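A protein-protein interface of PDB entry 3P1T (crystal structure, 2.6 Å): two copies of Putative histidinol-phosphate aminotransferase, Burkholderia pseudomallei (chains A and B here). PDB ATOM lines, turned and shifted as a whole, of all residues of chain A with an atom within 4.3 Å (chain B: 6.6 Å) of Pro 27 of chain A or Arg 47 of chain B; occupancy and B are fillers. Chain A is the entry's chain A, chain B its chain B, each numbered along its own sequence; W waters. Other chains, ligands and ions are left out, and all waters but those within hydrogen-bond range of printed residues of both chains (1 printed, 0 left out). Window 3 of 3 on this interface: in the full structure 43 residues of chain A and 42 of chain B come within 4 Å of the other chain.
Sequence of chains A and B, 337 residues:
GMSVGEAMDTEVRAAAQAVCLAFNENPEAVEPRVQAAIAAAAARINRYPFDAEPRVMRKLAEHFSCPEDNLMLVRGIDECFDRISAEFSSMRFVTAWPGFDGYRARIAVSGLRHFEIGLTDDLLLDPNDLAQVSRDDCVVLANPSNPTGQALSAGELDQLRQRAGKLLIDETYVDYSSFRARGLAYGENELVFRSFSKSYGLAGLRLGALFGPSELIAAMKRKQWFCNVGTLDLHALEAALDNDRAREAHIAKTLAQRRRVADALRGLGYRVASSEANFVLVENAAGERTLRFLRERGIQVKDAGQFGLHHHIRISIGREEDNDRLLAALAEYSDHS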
ATOM      1  N   GLU A  25      15.224  18.373 -15.528  1.00  0.00           N
ATOM      2  CA  GLU A  25      14.946  18.813 -14.163  1.00  0.00           C
ATOM      3  C   GLU A  25      14.226  20.166 -14.162  1.00  0.00           C
ATOM      4  O   GLU A  25      14.326  20.932 -15.135  1.00  0.00           O
ATOM      5  CB  GLU A  25      16.261  18.905 -13.358  1.00  0.00           C
ATOM      6  CG  GLU A  25      16.964  17.570 -13.115  1.00  0.00           C
ATOM      7  CD  GLU A  25      18.455  17.655 -12.843  1.00  0.00           C
ATOM      8  OE1 GLU A  25      19.145  18.438 -13.534  1.00  0.00           O
ATOM      9  OE2 GLU A  25      18.948  16.885 -11.988  1.00  0.00           O
ATOM     10  N   ASN A  26      13.485  20.463 -13.076  1.00  0.00           N
ATOM     11  CA  ASN A  26      12.850  21.779 -12.898  1.00  0.00           C
ATOM     12  C   ASN A  26      13.995  22.751 -12.575  1.00  0.00           C
ATOM     13  O   ASN A  26      14.723  22.480 -11.616  1.00  0.00           O
ATOM     14  CB  ASN A  26      11.752  21.734 -11.826  1.00  0.00           C
ATOM     15  CG  ASN A  26      11.043  23.038 -11.592  1.00  0.00           C
ATOM     16  OD1 ASN A  26      11.645  24.109 -11.512  1.00  0.00           O
ATOM     17  ND2 ASN A  26       9.745  22.970 -11.391  1.00  0.00           N
ATOM     18  N   PRO A  27      14.253  23.805 -13.399  1.00  0.00           N
ATOM     19  CA  PRO A  27      15.448  24.639 -13.174  1.00  0.00           C
ATOM     20  C   PRO A  27      15.270  25.740 -12.134  1.00  0.00           C
ATOM     21  O   PRO A  27      16.261  26.395 -11.771  1.00  0.00           O
ATOM     22  CB  PRO A  27      15.678  25.264 -14.547  1.00  0.00           C
ATOM     23  CG  PRO A  27      14.321  25.413 -15.113  1.00  0.00           C
ATOM     24  CD  PRO A  27      13.538  24.226 -14.624  1.00  0.00           C
ATOM     25  N   GLU A  28      14.026  25.954 -11.661  1.00  0.00           N
ATOM     26  CA  GLU A  28      13.695  27.000 -10.687  1.00  0.00           C
ATOM     27  C   GLU A  28      14.233  26.681  -9.314  1.00  0.00           C
ATOM     28  O   GLU A  28      14.473  25.512  -8.987  1.00  0.00           O
ATOM     29  CB  GLU A  28      12.166  27.222 -10.580  1.00  0.00           C
ATOM     30  CG  GLU A  28      11.426  27.390 -11.904  1.00  0.00           C
ATOM     31  CD  GLU A  28      11.925  28.421 -12.906  1.00  0.00           C
ATOM     32  OE1 GLU A  28      12.485  29.463 -12.489  1.00  0.00           O
ATOM     33  OE2 GLU A  28      11.721  28.190 -14.119  1.00  0.00           O
ATOM     34  N   ALA A  29      14.388  27.724  -8.496  1.00  0.00           N
ATOM     35  CA  ALA A  29      14.801  27.575  -7.106  1.00  0.00           C
ATOM     36  C   ALA A  29      13.664  26.932  -6.305  1.00  0.00           C
ATOM     37  O   ALA A  29      12.489  27.149  -6.634  1.00  0.00           O
ATOM     38  CB  ALA A  29      15.178  28.930  -6.531  1.00  0.00           C
ATOM     39  N   GLY A 204      14.886  14.874  -6.925  1.00  0.00           N
ATOM     40  CA  GLY A 204      15.801  14.270  -5.974  1.00  0.00           C
ATOM     41  C   GLY A 204      15.147  13.341  -4.979  1.00  0.00           C
ATOM     42  O   GLY A 204      15.861  12.657  -4.244  1.00  0.00           O
ATOM     43  N   HIS A 250       6.125  27.994 -13.726  1.00  0.00           N
ATOM     44  CA  HIS A 250       7.176  27.163 -14.308  1.00  0.00           C
ATOM     45  C   HIS A 250       6.681  26.542 -15.617  1.00  0.00           C
ATOM     46  O   HIS A 250       7.430  26.509 -16.590  1.00  0.00           O
ATOM     47  CB  HIS A 250       7.636  26.077 -13.305  1.00  0.00           C
ATOM     48  CG  HIS A 250       8.267  24.893 -13.947  1.00  0.00           C
ATOM     49  ND1 HIS A 250       9.535  24.954 -14.481  1.00  0.00           N
ATOM     50  CD2 HIS A 250       7.774  23.649 -14.142  1.00  0.00           C
ATOM     51  CE1 HIS A 250       9.780  23.750 -14.978  1.00  0.00           C
ATOM     52  NE2 HIS A 250       8.750  22.935 -14.803  1.00  0.00           N
ATOM     53  N   GLY A 318      15.516  24.961 -19.874  1.00  0.00           N
ATOM     54  CA  GLY A 318      15.842  25.493 -18.550  1.00  0.00           C
ATOM     55  C   GLY A 318      15.352  26.913 -18.365  1.00  0.00           C
ATOM     56  O   GLY A 318      14.376  27.318 -19.003  1.00  0.00           O
ATOM     57  N   ARG A 319      16.027  27.691 -17.506  1.00  0.00           N
ATOM     58  CA  ARG A 319      15.677  29.109 -17.368  1.00  0.00           C
ATOM     59  C   ARG A 319      16.141  29.892 -18.630  1.00  0.00           C
ATOM     60  O   ARG A 319      16.930  29.387 -19.429  1.00  0.00           O
ATOM     61  CB  ARG A 319      16.281  29.705 -16.092  1.00  0.00           C
ATOM     62  CG  ARG A 319      15.474  29.450 -14.827  1.00  0.00           C
ATOM     63  CD  ARG A 319      16.281  29.753 -13.574  1.00  0.00           C
ATOM     64  NE  ARG A 319      17.298  28.720 -13.335  1.00  0.00           N
ATOM     65  CZ  ARG A 319      18.598  28.855 -13.585  1.00  0.00           C
ATOM     66  NH1 ARG A 319      19.078  30.006 -14.039  1.00  0.00           N
ATOM     67  NH2 ARG A 319      19.433  27.850 -13.349  1.00  0.00           N
ATOM     68  N   ARG B  44      18.154  21.810  -2.911  1.00  0.00           N
ATOM     69  CA  ARG B  44      18.547  21.115  -4.143  1.00  0.00           C
ATOM     70  C   ARG B  44      17.695  19.846  -4.424  1.00  0.00           C
ATOM     71  O   ARG B  44      18.120  19.007  -5.211  1.00  0.00           O
ATOM     72  CB  ARG B  44      20.032  20.724  -4.056  1.00  0.00           C
ATOM     73  CG  ARG B  44      20.974  21.911  -4.078  1.00  0.00           C
ATOM     74  CD  ARG B  44      22.390  21.458  -3.812  1.00  0.00           C
ATOM     75  NE  ARG B  44      23.064  22.317  -2.841  1.00  0.00           N
ATOM     76  N   ILE B  45      16.476  19.750  -3.861  1.00  0.00           N
ATOM     77  CA  ILE B  45      15.595  18.584  -4.049  1.00  0.00           C
ATOM     78  C   ILE B  45      15.085  18.501  -5.510  1.00  0.00           C
ATOM     79  O   ILE B  45      14.581  17.445  -5.901  1.00  0.00           O
ATOM     80  CB  ILE B  45      14.402  18.552  -3.060  1.00  0.00           C
ATOM     81  CG1 ILE B  45      13.491  19.785  -3.222  1.00  0.00           C
ATOM     82  CG2 ILE B  45      14.899  18.363  -1.639  1.00  0.00           C
ATOM     83  CD1 ILE B  45      12.243  19.755  -2.411  1.00  0.00           C
ATOM     84  N   ASN B  46      15.277  19.564  -6.318  1.00  0.00           N
ATOM     85  CA  ASN B  46      14.848  19.611  -7.722  1.00  0.00           C
ATOM     86  C   ASN B  46      15.821  18.869  -8.652  1.00  0.00           C
ATOM     87  O   ASN B  46      15.509  18.702  -9.837  1.00  0.00           O
ATOM     88  CB  ASN B  46      14.709  21.078  -8.187  1.00  0.00           C
ATOM     89  CG  ASN B  46      15.966  21.918  -8.117  1.00  0.00           C
ATOM     90  OD1 ASN B  46      16.734  21.884  -7.157  1.00  0.00           O
ATOM     91  ND2 ASN B  46      16.169  22.748  -9.112  1.00  0.00           N
ATOM     92  N   ARG B  47      16.994  18.453  -8.129  1.00  0.00           N
ATOM     93  CA  ARG B  47      18.044  17.779  -8.885  1.00  0.00           C
ATOM     94  C   ARG B  47      18.287  16.358  -8.390  1.00  0.00           C
ATOM     95  O   ARG B  47      18.240  16.105  -7.180  1.00  0.00           O
ATOM     96  CB  ARG B  47      19.372  18.570  -8.780  1.00  0.00           C
ATOM     97  CG  ARG B  47      19.351  20.061  -9.166  1.00  0.00           C
ATOM     98  CD  ARG B  47      19.286  20.328 -10.652  1.00  0.00           C
ATOM     99  NE  ARG B  47      19.249  21.765 -10.925  1.00  0.00           N
ATOM    100  CZ  ARG B  47      19.131  22.294 -12.135  1.00  0.00           C
ATOM    101  NH1 ARG B  47      19.020  21.510 -13.204  1.00  0.00           N
ATOM    102  NH2 ARG B  47      19.107  23.611 -12.286  1.00  0.00           N
ATOM    103  N   TYR B  48      18.624  15.444  -9.315  1.00  0.00           N
ATOM    104  CA  TYR B  48      18.935  14.058  -8.950  1.00  0.00           C
ATOM    105  C   TYR B  48      20.240  14.025  -8.104  1.00  0.00           C
ATOM    106  O   TYR B  48      21.186  14.761  -8.425  1.00  0.00           O
ATOM    107  CB  TYR B  48      19.037  13.159 -10.194  1.00  0.00           C
ATOM    108  CG  TYR B  48      17.707  12.914 -10.877  1.00  0.00           C
ATOM    109  CD1 TYR B  48      16.799  11.983 -10.369  1.00  0.00           C
ATOM    110  CD2 TYR B  48      17.374  13.575 -12.058  1.00  0.00           C
ATOM    111  CE1 TYR B  48      15.571  11.753 -10.991  1.00  0.00           C
ATOM    112  CE2 TYR B  48      16.150  13.348 -12.697  1.00  0.00           C
ATOM    113  CZ  TYR B  48      15.256  12.425 -12.166  1.00  0.00           C
ATOM    114  OH  TYR B  48      14.056  12.164 -12.798  1.00  0.00           O
ATOM    115  N   PRO B  49      20.292  13.224  -6.996  1.00  0.00           N
ATOM    116  CA  PRO B  49      21.495  13.228  -6.145  1.00  0.00           C
ATOM    117  C   PRO B  49      22.611  12.345  -6.730  1.00  0.00           C
ATOM    118  O   PRO B  49      23.070  11.399  -6.076  1.00  0.00           O
ATOM    119  CB  PRO B  49      20.961  12.679  -4.815  1.00  0.00           C
ATOM    120  CG  PRO B  49      19.851  11.756  -5.192  1.00  0.00           C
ATOM    121  CD  PRO B  49      19.254  12.303  -6.462  1.00  0.00           C
ATOM    122  N   PHE B  50      23.064  12.661  -7.960  1.00  0.00           N
ATOM    123  CA  PHE B  50      24.066  11.876  -8.684  1.00  0.00           C
ATOM    124  C   PHE B  50      25.431  11.868  -7.992  1.00  0.00           C
ATOM    125  O   PHE B  50      26.159  10.886  -8.125  1.00  0.00           O
ATOM    126  CB  PHE B  50      24.242  12.384 -10.126  1.00  0.00           C
ATOM    127  CG  PHE B  50      23.091  12.094 -11.066  1.00  0.00           C
ATOM    128  CD1 PHE B  50      22.615  10.800 -11.226  1.00  0.00           C
ATOM    129  CD2 PHE B  50      22.543  13.101 -11.858  1.00  0.00           C
ATOM    130  CE1 PHE B  50      21.573  10.526 -12.118  1.00  0.00           C
ATOM    131  CE2 PHE B  50      21.497  12.827 -12.743  1.00  0.00           C
ATOM    132  CZ  PHE B  50      21.015  11.540 -12.862  1.00  0.00           C
ATOM    133  N   THR B 231      17.656  12.444  -1.998  1.00  0.00           N
ATOM    134  CA  THR B 231      18.633  13.437  -1.545  1.00  0.00           C
ATOM    135  C   THR B 231      18.420  13.826  -0.042  1.00  0.00           C
ATOM    136  O   THR B 231      19.409  13.960   0.661  1.00  0.00           O
ATOM    137  CB  THR B 231      18.610  14.684  -2.445  1.00  0.00           C
ATOM    138  OG1 THR B 231      19.464  15.669  -1.877  1.00  0.00           O
ATOM    139  CG2 THR B 231      17.219  15.280  -2.644  1.00  0.00           C
HETATM  140  O   HOH W   1      21.233  16.055 -10.834  1.00  0.00           O
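OE2 of Glu 25 of chain A sits at hydrogen-bond distance from N of Tyr 48 of chain B. The backbone carbonyl oxygen (O) of Ile 45 of chain B lies within hydrogen-bond range of the backbone NH (N) of Gly 204 of chain A. The backbone carbonyl oxygen of Gly 204 of chain A lies within hydrogen-bond range of the backbone NH of Thr 231 of chain B. The side-chain carboxylate (OE1) of Glu 25 of chain A is in salt-bridge range of the guanidinium group (NH1) of Arg 47 of chain B (3.1 Å). The backbone carbonyl oxygen of Glu 28 of chain A lies within hydrogen-bond range of the side-chain amide nitrogen of Asn 46 of chain B. The side-chain amide nitrogen of Asn 46 of chain B is in hydrogen-bond range of the backbone carbonyl oxygen of Asn 26 of chain A, 2.9 Å away.
Asn 46 of chain B touches Glu 25 of chain A (O to CB, 3.6 Å). Pro 27 of chain A touches Arg 47 of chain B. Arg 47 of chain B touches Gly 204 of chain A (O to CA, 3.3 Å).
Printed residues of chain B within 4 Å of Glu 25 of chain A: Asn 46, Arg 47 and Tyr 48. Pro 27 of chain A touches just one residue of chain B: Arg 47 (3.9 Å). Printed residues of chain B within 4 Å of Glu 28 of chain A: Asn 46 (3.2 Å). His 250 of chain A touches none of the printed residues of chain B. Gly 318 of chain A touches none of the printed residues of chain B. Printed residues of chain A within 4 Å of Ile 45 of chain B: Gly 204 (2.8 Å). Of the printed residues of chain A, Asn 46 of chain B touches Glu 25 (3.6 Å), Asn 26 (2.9 Å) and Glu 28 (3.2 Å). Arg 47 of chain B touches just these residues of chain A: Glu 25, Pro 27 and Gly 204.
Water W1 bridges the side-chain carboxylate (OE2) of Glu 25 of chain A (2.7 Å) and the backbone carbonyl oxygen (O) of Tyr 48 of chain B (2.7 Å).
No position is printed for both chains. Of the 9 pairs that touch across the chains among the printed residues, none has its exchanged pair printed and touching as well.
The side-chain amide oxygen (OD1) of Asn 26 of chain A is in hydrogen-bond range of the backbone NH (N) of Glu 28 of chain A, at 3.0 Å. The backbone carbonyl oxygen (O) of Pro 27 of chain A lies within hydrogen-bond range of the guanidinium group (NE) of Arg 319 of chain A.
Of the 8 printed residues of chain B, 5 touch a printed residue of chain A. Printed residues of chain B that touch a printed residue of chain A: Ile 45, Asn 46, Arg 47, Tyr 48 and Thr 231. Along chain B the printed residues that touch a printed residue of chain A span positions 45 to 231. Of the 9 printed residues of chain A, 5 touch a printed residue of chain B. Among the printed residues, Asp or Glu carboxylates within 4 Å of a Lys or Arg side-chain nitrogen of the other chain: Glu 25 of chain A with Arg 47 of chain B (3.1 Å).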
